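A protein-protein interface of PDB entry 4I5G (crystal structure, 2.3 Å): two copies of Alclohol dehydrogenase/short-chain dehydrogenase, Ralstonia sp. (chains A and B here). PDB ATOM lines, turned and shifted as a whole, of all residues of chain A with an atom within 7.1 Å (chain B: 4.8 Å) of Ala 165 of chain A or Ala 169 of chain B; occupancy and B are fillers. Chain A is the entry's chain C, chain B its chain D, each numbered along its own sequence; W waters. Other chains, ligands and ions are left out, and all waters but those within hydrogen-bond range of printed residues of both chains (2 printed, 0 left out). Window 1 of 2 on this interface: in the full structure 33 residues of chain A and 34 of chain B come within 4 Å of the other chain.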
ATOM      1  N   TYR A 117     -10.790   1.011  15.635  1.00  0.00           N
ATOM      2  CA  TYR A 117     -12.018   0.285  15.450  1.00  0.00           C
ATOM      3  C   TYR A 117     -13.312   1.115  15.335  1.00  0.00           C
ATOM      4  O   TYR A 117     -14.121   0.868  14.428  1.00  0.00           O
ATOM      5  CB  TYR A 117     -12.169  -0.758  16.537  1.00  0.00           C
ATOM      6  CG  TYR A 117     -13.484  -1.454  16.475  1.00  0.00           C
ATOM      7  CD1 TYR A 117     -14.598  -0.951  17.152  1.00  0.00           C
ATOM      8  CD2 TYR A 117     -13.615  -2.630  15.724  1.00  0.00           C
ATOM      9  CE1 TYR A 117     -15.838  -1.588  17.068  1.00  0.00           C
ATOM     10  CE2 TYR A 117     -14.835  -3.300  15.636  1.00  0.00           C
ATOM     11  CZ  TYR A 117     -15.945  -2.778  16.276  1.00  0.00           C
ATOM     12  OH  TYR A 117     -17.110  -3.499  16.180  1.00  0.00           O
ATOM     13  N   THR A 120     -13.546   3.144  12.004  1.00  0.00           N
ATOM     14  CA  THR A 120     -13.855   2.257  10.916  1.00  0.00           C
ATOM     15  C   THR A 120     -15.346   1.797  10.832  1.00  0.00           C
ATOM     16  O   THR A 120     -15.960   1.821   9.738  1.00  0.00           O
ATOM     17  CB  THR A 120     -12.940   1.036  10.984  1.00  0.00           C
ATOM     18  OG1 THR A 120     -11.667   1.460  10.583  1.00  0.00           O
ATOM     19  CG2 THR A 120     -13.404  -0.075   9.986  1.00  0.00           C
ATOM     20  N   PHE A 121     -15.900   1.372  11.963  1.00  0.00           N
ATOM     21  CA  PHE A 121     -17.217   0.801  11.985  1.00  0.00           C
ATOM     22  C   PHE A 121     -18.285   1.871  12.062  1.00  0.00           C
ATOM     23  O   PHE A 121     -19.416   1.687  11.536  1.00  0.00           O
ATOM     24  CB  PHE A 121     -17.339  -0.265  13.072  1.00  0.00           C
ATOM     25  CG  PHE A 121     -16.894  -1.646  12.605  1.00  0.00           C
ATOM     26  CD1 PHE A 121     -15.539  -1.945  12.475  1.00  0.00           C
ATOM     27  CD2 PHE A 121     -17.844  -2.611  12.268  1.00  0.00           C
ATOM     28  CE1 PHE A 121     -15.094  -3.200  12.075  1.00  0.00           C
ATOM     29  CE2 PHE A 121     -17.423  -3.882  11.799  1.00  0.00           C
ATOM     30  CZ  PHE A 121     -16.040  -4.160  11.705  1.00  0.00           C
ATOM     31  N   VAL A 125     -20.318   1.217   8.820  1.00  0.00           N
ATOM     32  CA  VAL A 125     -21.453   0.327   9.175  1.00  0.00           C
ATOM     33  C   VAL A 125     -22.479   1.122   9.951  1.00  0.00           C
ATOM     34  O   VAL A 125     -23.663   1.163   9.554  1.00  0.00           O
ATOM     35  CB  VAL A 125     -21.006  -0.971   9.932  1.00  0.00           C
ATOM     36  CG1 VAL A 125     -22.143  -1.932  10.125  1.00  0.00           C
ATOM     37  CG2 VAL A 125     -19.891  -1.721   9.166  1.00  0.00           C
ATOM     38  N   ALA A 152     -11.982  -6.113  -0.600  1.00  0.00           N
ATOM     39  CA  ALA A 152     -11.367  -6.402   0.727  1.00  0.00           C
ATOM     40  C   ALA A 152     -12.284  -7.250   1.499  1.00  0.00           C
ATOM     41  O   ALA A 152     -11.822  -8.083   2.313  1.00  0.00           O
ATOM     42  CB  ALA A 152     -11.065  -5.134   1.478  1.00  0.00           C
ATOM     43  N   GLY A 153     -13.587  -7.126   1.199  1.00  0.00           N
ATOM     44  CA  GLY A 153     -14.627  -7.763   1.994  1.00  0.00           C
ATOM     45  C   GLY A 153     -14.547  -9.297   1.798  1.00  0.00           C
ATOM     46  O   GLY A 153     -15.161 -10.094   2.565  1.00  0.00           O
ATOM     47  N   HIS A 160      -5.716  -4.882   6.960  1.00  0.00           N
ATOM     48  CA  HIS A 160      -7.078  -4.425   6.648  1.00  0.00           C
ATOM     49  C   HIS A 160      -8.131  -4.984   7.551  1.00  0.00           C
ATOM     50  O   HIS A 160      -9.347  -4.916   7.200  1.00  0.00           O
ATOM     51  CB  HIS A 160      -7.483  -4.716   5.218  1.00  0.00           C
ATOM     52  CG  HIS A 160      -6.630  -3.989   4.233  1.00  0.00           C
ATOM     53  ND1 HIS A 160      -5.251  -4.146   4.195  1.00  0.00           N
ATOM     54  CD2 HIS A 160      -6.957  -3.057   3.261  1.00  0.00           C
ATOM     55  CE1 HIS A 160      -4.756  -3.351   3.236  1.00  0.00           C
ATOM     56  NE2 HIS A 160      -5.799  -2.675   2.671  1.00  0.00           N
ATOM     57  N   ASP A 161      -7.704  -5.483   8.708  1.00  0.00           N
ATOM     58  CA  ASP A 161      -8.659  -6.126   9.594  1.00  0.00           C
ATOM     59  C   ASP A 161     -10.080  -5.483   9.693  1.00  0.00           C
ATOM     60  O   ASP A 161     -11.075  -6.068   9.214  1.00  0.00           O
ATOM     61  CB  ASP A 161      -8.060  -6.267  10.970  1.00  0.00           C
ATOM     62  CG  ASP A 161      -6.664  -6.840  10.951  1.00  0.00           C
ATOM     63  OD1 ASP A 161      -5.780  -6.427  10.125  1.00  0.00           O
ATOM     64  OD2 ASP A 161      -6.421  -7.668  11.831  1.00  0.00           O
ATOM     65  N   THR A 162     -10.180  -4.297  10.278  1.00  0.00           N
ATOM     66  CA  THR A 162     -11.477  -3.647  10.536  1.00  0.00           C
ATOM     67  C   THR A 162     -12.177  -3.204   9.253  1.00  0.00           C
ATOM     68  O   THR A 162     -13.398  -3.368   9.112  1.00  0.00           O
ATOM     69  CB  THR A 162     -11.370  -2.473  11.591  1.00  0.00           C
ATOM     70  OG1 THR A 162     -10.556  -1.411  11.102  1.00  0.00           O
ATOM     71  CG2 THR A 162     -10.731  -2.984  12.900  1.00  0.00           C
ATOM     72  N   TYR A 163     -11.412  -2.683   8.284  1.00  0.00           N
ATOM     73  CA  TYR A 163     -12.011  -2.255   7.023  1.00  0.00           C
ATOM     74  C   TYR A 163     -12.596  -3.434   6.267  1.00  0.00           C
ATOM     75  O   TYR A 163     -13.712  -3.334   5.794  1.00  0.00           O
ATOM     76  CB  TYR A 163     -11.003  -1.512   6.139  1.00  0.00           C
ATOM     77  CG  TYR A 163     -11.557  -1.125   4.825  1.00  0.00           C
ATOM     78  CD1 TYR A 163     -12.213   0.072   4.667  1.00  0.00           C
ATOM     79  CD2 TYR A 163     -11.411  -1.952   3.697  1.00  0.00           C
ATOM     80  CE1 TYR A 163     -12.770   0.450   3.458  1.00  0.00           C
ATOM     81  CE2 TYR A 163     -11.953  -1.559   2.427  1.00  0.00           C
ATOM     82  CZ  TYR A 163     -12.602  -0.361   2.352  1.00  0.00           C
ATOM     83  OH  TYR A 163     -13.093   0.061   1.156  1.00  0.00           O
ATOM     84  N   SER A 164     -11.882  -4.545   6.133  1.00  0.00           N
ATOM     85  CA  SER A 164     -12.463  -5.768   5.428  1.00  0.00           C
ATOM     86  C   SER A 164     -13.749  -6.273   6.142  1.00  0.00           C
ATOM     87  O   SER A 164     -14.792  -6.548   5.516  1.00  0.00           O
ATOM     88  CB  SER A 164     -11.374  -6.848   5.462  1.00  0.00           C
ATOM     89  OG  SER A 164     -10.273  -6.306   4.788  1.00  0.00           O
ATOM     90  N   ALA A 165     -13.689  -6.345   7.474  1.00  0.00           N
ATOM     91  CA  ALA A 165     -14.812  -6.840   8.246  1.00  0.00           C
ATOM     92  C   ALA A 165     -16.027  -5.934   8.093  1.00  0.00           C
ATOM     93  O   ALA A 165     -17.171  -6.398   7.863  1.00  0.00           O
ATOM     94  CB  ALA A 165     -14.429  -6.990   9.730  1.00  0.00           C
ATOM     95  N   ALA A 166     -15.788  -4.636   8.120  1.00  0.00           N
ATOM     96  CA  ALA A 166     -16.860  -3.700   7.942  1.00  0.00           C
ATOM     97  C   ALA A 166     -17.338  -3.757   6.504  1.00  0.00           C
ATOM     98  O   ALA A 166     -18.548  -3.621   6.251  1.00  0.00           O
ATOM     99  CB  ALA A 166     -16.372  -2.303   8.288  1.00  0.00           C
ATOM    100  N   LYS A 167     -16.448  -3.955   5.522  1.00  0.00           N
ATOM    101  CA  LYS A 167     -17.052  -3.993   4.132  1.00  0.00           C
ATOM    102  C   LYS A 167     -17.815  -5.357   3.914  1.00  0.00           C
ATOM    103  O   LYS A 167     -18.680  -5.453   3.134  1.00  0.00           O
ATOM    104  CB  LYS A 167     -16.005  -3.687   3.027  1.00  0.00           C
ATOM    105  CG  LYS A 167     -15.556  -2.217   2.881  1.00  0.00           C
ATOM    106  CD  LYS A 167     -16.750  -1.312   2.862  1.00  0.00           C
ATOM    107  CE  LYS A 167     -16.339   0.038   2.298  1.00  0.00           C
ATOM    108  NZ  LYS A 167     -17.403   1.018   2.544  1.00  0.00           N
ATOM    109  N   ALA A 168     -17.497  -6.396   4.664  1.00  0.00           N
ATOM    110  CA  ALA A 168     -18.209  -7.682   4.531  1.00  0.00           C
ATOM    111  C   ALA A 168     -19.584  -7.499   5.211  1.00  0.00           C
ATOM    112  O   ALA A 168     -20.595  -8.069   4.753  1.00  0.00           O
ATOM    113  CB  ALA A 168     -17.402  -8.830   5.221  1.00  0.00           C
ATOM    114  N   ALA A 169     -19.599  -6.751   6.329  1.00  0.00           N
ATOM    115  CA  ALA A 169     -20.866  -6.389   7.010  1.00  0.00           C
ATOM    116  C   ALA A 169     -21.784  -5.584   6.049  1.00  0.00           C
ATOM    117  O   ALA A 169     -22.991  -5.854   5.950  1.00  0.00           O
ATOM    118  CB  ALA A 169     -20.608  -5.623   8.307  1.00  0.00           C
ATOM    119  N   VAL A 170     -21.199  -4.636   5.327  1.00  0.00           N
ATOM    120  CA  VAL A 170     -21.939  -3.902   4.335  1.00  0.00           C
ATOM    121  C   VAL A 170     -22.557  -4.841   3.268  1.00  0.00           C
ATOM    122  O   VAL A 170     -23.673  -4.624   2.862  1.00  0.00           O
ATOM    123  CB  VAL A 170     -21.084  -2.805   3.624  1.00  0.00           C
ATOM    124  CG1 VAL A 170     -21.873  -2.319   2.372  1.00  0.00           C
ATOM    125  CG2 VAL A 170     -20.723  -1.658   4.574  1.00  0.00           C
ATOM    126  N   ARG A 171     -21.818  -5.844   2.780  1.00  0.00           N
ATOM    127  CA  ARG A 171     -22.375  -6.781   1.744  1.00  0.00           C
ATOM    128  C   ARG A 171     -23.587  -7.590   2.320  1.00  0.00           C
ATOM    129  O   ARG A 171     -24.593  -7.791   1.668  1.00  0.00           O
ATOM    130  CB  ARG A 171     -21.229  -7.687   1.167  1.00  0.00           C
ATOM    131  CG  ARG A 171     -21.596  -8.591  -0.041  1.00  0.00           C
ATOM    132  CD  ARG A 171     -22.258  -9.899   0.404  1.00  0.00           C
ATOM    133  NE  ARG A 171     -22.882 -10.586  -0.707  1.00  0.00           N
ATOM    134  CZ  ARG A 171     -24.050 -10.247  -1.265  1.00  0.00           C
ATOM    135  NH1 ARG A 171     -24.739  -9.188  -0.822  1.00  0.00           N
ATOM    136  NH2 ARG A 171     -24.532 -10.962  -2.325  1.00  0.00           N
ATOM    137  N   SER A 172     -23.486  -8.014   3.576  1.00  0.00           N
ATOM    138  CA  SER A 172     -24.545  -8.691   4.260  1.00  0.00           C
ATOM    139  C   SER A 172     -25.813  -7.815   4.369  1.00  0.00           C
ATOM    140  O   SER A 172     -26.924  -8.353   4.235  1.00  0.00           O
ATOM    141  CB  SER A 172     -24.118  -9.103   5.667  1.00  0.00           C
ATOM    142  OG  SER A 172     -25.290  -9.413   6.424  1.00  0.00           O
ATOM    143  N   VAL B 125     -18.086  -8.541  17.260  1.00  0.00           N
ATOM    144  CA  VAL B 125     -16.928  -8.052  16.441  1.00  0.00           C
ATOM    145  C   VAL B 125     -15.815  -7.410  17.287  1.00  0.00           C
ATOM    146  O   VAL B 125     -14.629  -7.903  17.270  1.00  0.00           O
ATOM    147  CB  VAL B 125     -17.377  -7.080  15.305  1.00  0.00           C
ATOM    148  CG1 VAL B 125     -16.172  -6.619  14.470  1.00  0.00           C
ATOM    149  CG2 VAL B 125     -18.437  -7.720  14.447  1.00  0.00           C
ATOM    150  N   ALA B 165     -24.788  -8.937   9.775  1.00  0.00           N
ATOM    151  CA  ALA B 165     -23.695  -8.094   9.328  1.00  0.00           C
ATOM    152  C   ALA B 165     -22.447  -8.339  10.231  1.00  0.00           C
ATOM    153  O   ALA B 165     -21.326  -8.457   9.806  1.00  0.00           O
ATOM    154  CB  ALA B 165     -24.154  -6.605   9.347  1.00  0.00           C
ATOM    155  N   ALA B 166     -22.694  -8.397  11.514  1.00  0.00           N
ATOM    156  CA  ALA B 166     -21.721  -8.696  12.484  1.00  0.00           C
ATOM    157  C   ALA B 166     -21.026 -10.084  12.194  1.00  0.00           C
ATOM    158  O   ALA B 166     -19.780 -10.177  12.171  1.00  0.00           O
ATOM    159  CB  ALA B 166     -22.422  -8.668  13.850  1.00  0.00           C
ATOM    160  N   LYS B 167     -21.810 -11.150  12.009  1.00  0.00           N
ATOM    161  CA  LYS B 167     -21.205 -12.452  11.777  1.00  0.00           C
ATOM    162  C   LYS B 167     -20.517 -12.507  10.375  1.00  0.00           C
ATOM    163  O   LYS B 167     -19.558 -13.277  10.151  1.00  0.00           O
ATOM    164  CB  LYS B 167     -22.269 -13.566  11.910  1.00  0.00           C
ATOM    165  CG  LYS B 167     -22.794 -13.727  13.348  1.00  0.00           C
ATOM    166  CD  LYS B 167     -21.617 -13.832  14.295  1.00  0.00           C
ATOM    167  CE  LYS B 167     -22.018 -14.558  15.562  1.00  0.00           C
ATOM    168  NZ  LYS B 167     -20.901 -14.588  16.565  1.00  0.00           N
ATOM    169  N   ALA B 168     -20.995 -11.697   9.419  1.00  0.00           N
ATOM    170  CA  ALA B 168     -20.218 -11.603   8.165  1.00  0.00           C
ATOM    171  C   ALA B 168     -18.860 -10.900   8.450  1.00  0.00           C
ATOM    172  O   ALA B 168     -17.831 -11.318   7.865  1.00  0.00           O
ATOM    173  CB  ALA B 168     -20.981 -10.943   7.033  1.00  0.00           C
ATOM    174  N   ALA B 169     -18.841  -9.915   9.381  1.00  0.00           N
ATOM    175  CA  ALA B 169     -17.577  -9.271   9.770  1.00  0.00           C
ATOM    176  C   ALA B 169     -16.625 -10.321  10.418  1.00  0.00           C
ATOM    177  O   ALA B 169     -15.448 -10.359  10.130  1.00  0.00           O
ATOM    178  CB  ALA B 169     -17.859  -8.086  10.727  1.00  0.00           C
ATOM    179  N   VAL B 170     -17.139 -11.216  11.269  1.00  0.00           N
ATOM    180  CA  VAL B 170     -16.319 -12.339  11.849  1.00  0.00           C
ATOM    181  C   VAL B 170     -15.750 -13.185  10.736  1.00  0.00           C
ATOM    182  O   VAL B 170     -14.591 -13.497  10.741  1.00  0.00           O
ATOM    183  CB  VAL B 170     -17.121 -13.262  12.785  1.00  0.00           C
ATOM    184  CG1 VAL B 170     -16.326 -14.466  13.165  1.00  0.00           C
ATOM    185  CG2 VAL B 170     -17.504 -12.529  14.099  1.00  0.00           C
ATOM    186  N   ARG B 171     -16.553 -13.599   9.771  1.00  0.00           N
ATOM    187  CA  ARG B 171     -16.015 -14.547   8.753  1.00  0.00           C
ATOM    188  C   ARG B 171     -14.805 -13.871   7.992  1.00  0.00           C
ATOM    189  O   ARG B 171     -13.767 -14.470   7.779  1.00  0.00           O
ATOM    190  CB  ARG B 171     -17.132 -15.078   7.822  1.00  0.00           C
ATOM    191  CG  ARG B 171     -16.686 -16.101   6.759  1.00  0.00           C
ATOM    192  CD  ARG B 171     -15.973 -15.494   5.550  1.00  0.00           C
ATOM    193  NE  ARG B 171     -15.353 -16.553   4.745  1.00  0.00           N
ATOM    194  CZ  ARG B 171     -14.181 -17.180   5.041  1.00  0.00           C
ATOM    195  NH1 ARG B 171     -13.512 -16.918   6.152  1.00  0.00           N
ATOM    196  NH2 ARG B 171     -13.701 -18.155   4.253  1.00  0.00           N
ATOM    197  N   SER B 172     -14.946 -12.580   7.742  1.00  0.00           N
ATOM    198  CA  SER B 172     -13.868 -11.749   7.195  1.00  0.00           C
ATOM    199  C   SER B 172     -12.560 -11.761   8.022  1.00  0.00           C
ATOM    200  O   SER B 172     -11.472 -11.916   7.446  1.00  0.00           O
ATOM    201  CB  SER B 172     -14.360 -10.315   7.007  1.00  0.00           C
ATOM    202  OG  SER B 172     -13.301  -9.504   6.499  1.00  0.00           O
ATOM    203  N   LEU B 173     -12.661 -11.645   9.356  1.00  0.00           N
ATOM    204  CA  LEU B 173     -11.408 -11.605  10.209  1.00  0.00           C
ATOM    205  C   LEU B 173     -10.647 -12.966  10.161  1.00  0.00           C
ATOM    206  O   LEU B 173      -9.423 -13.017  10.209  1.00  0.00           O
ATOM    207  CB  LEU B 173     -11.736 -11.139  11.635  1.00  0.00           C
ATOM    208  CG  LEU B 173     -12.287  -9.741  11.903  1.00  0.00           C
ATOM    209  CD1 LEU B 173     -12.968  -9.600  13.266  1.00  0.00           C
ATOM    210  CD2 LEU B 173     -11.126  -8.767  11.821  1.00  0.00           C
HETATM  211  O   HOH W   1     -12.567 -10.223   4.188  1.00  0.00           O
HETATM  212  O   HOH W   2     -11.212  -8.765   8.356  1.00  0.00           O
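OG of Ser 172 of chain B lies close to O of Ser 164 of chain A, 3.5 Å away.
The side-chain hydroxyl (OG) of Ser 172 of chain B lies within hydrogen-bond range of the backbone NH (N) of Ala 165 of chain A (3.3 Å).
The side-chain hydroxyl of Ser 172 of chain A lies within hydrogen-bond range of the backbone NH of Ala 165 of chain B, at 3.4 Å.
O of Ala 152 of chain A lies close to OG of Ser 164 of chain A (3.4 Å).
OG of Ser 164 of chain A sits at hydrogen-bond distance from O of His 160 of chain A (2.9 Å).
Among the printed residues, pairs that only touch across the chains: Tyr 117 of chain A with Val 125 of chain B (3.7 Å), Phe 121 of chain A with Val 125 of chain B (3.7 Å), Asp 161 of chain A with Leu 173 of chain B (3.8 Å), Ala 165 of chain A with Ala 169 of chain B (3.4 Å), Ala 168 of chain A with Ala 168 of chain B (3.7 Å), Ala 168 of chain A with Ser 172 of chain B (3.8 Å), Ala 169 of chain A with Ala 165 of chain B (3.3 Å) and Ser 172 of chain A with Ala 168 of chain B (3.9 Å).
Ala 165 of chain A touches just these residues of chain B: Ala 169 and Ser 172.
Of chain A, only Ala 165 comes within 4 Å of Ala 169 of chain B.
Of the printed residues of chain B, Tyr 117 of chain A touches Val 125.
Of the printed residues of chain B, Asp 161 of chain A touches Leu 173.
Ala 166 of chain A touches none of the printed residues of chain B.
Val 125 of chain A touches none of the printed residues of chain B.
The nearest residue of chain A that does not touch Ala 169 of chain B is Phe 121 of chain A (4.4 Å).
Of the 19 printed residues of chain A, 8 touch a printed residue of chain B.
Hydrophobic or aromatic side chains of chain A that line the printed part of chain B: Tyr 117, Phe 121, Ala 165, Ala 168 and Ala 169.
Hydrophobic or aromatic side chains of chain B that line the printed part of chain A: Val 125, Ala 165, Ala 168, Ala 169 and Leu 173.
Among the printed residues, no Asp or Glu carboxylate lies within 4 Å of a Lys or Arg side-chain nitrogen of the other chain.
Ala 165 of chain A touches Ala 169 of chain B, and with the chains exchanged Ala 169 of chain A touches Ala 165 of chain B.
Ala 165 of chain A touches Ser 172 of chain B, and with the chains exchanged Ser 172 of chain A touches Ala 165 of chain B.
Ala 168 of chain B touches its own counterpart, Ala 168 of chain A.
Ala 168 of chain A touches Ser 172 of chain B, and with the chains exchanged Ser 172 of chain A touches Ala 168 of chain B.
Water W1 lies within hydrogen-bond range of OG of Ser 172 of chain B, O of Ala 152 of chain A and O of Gly 153 of chain A.
Water W2 lies within hydrogen-bond range of the backbone carbonyl oxygen (O) of Asp 161 of chain A, the side-chain hydroxyl (OG) of Ser 172 of chain B and the backbone NH (N) of Leu 173 of chain B.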
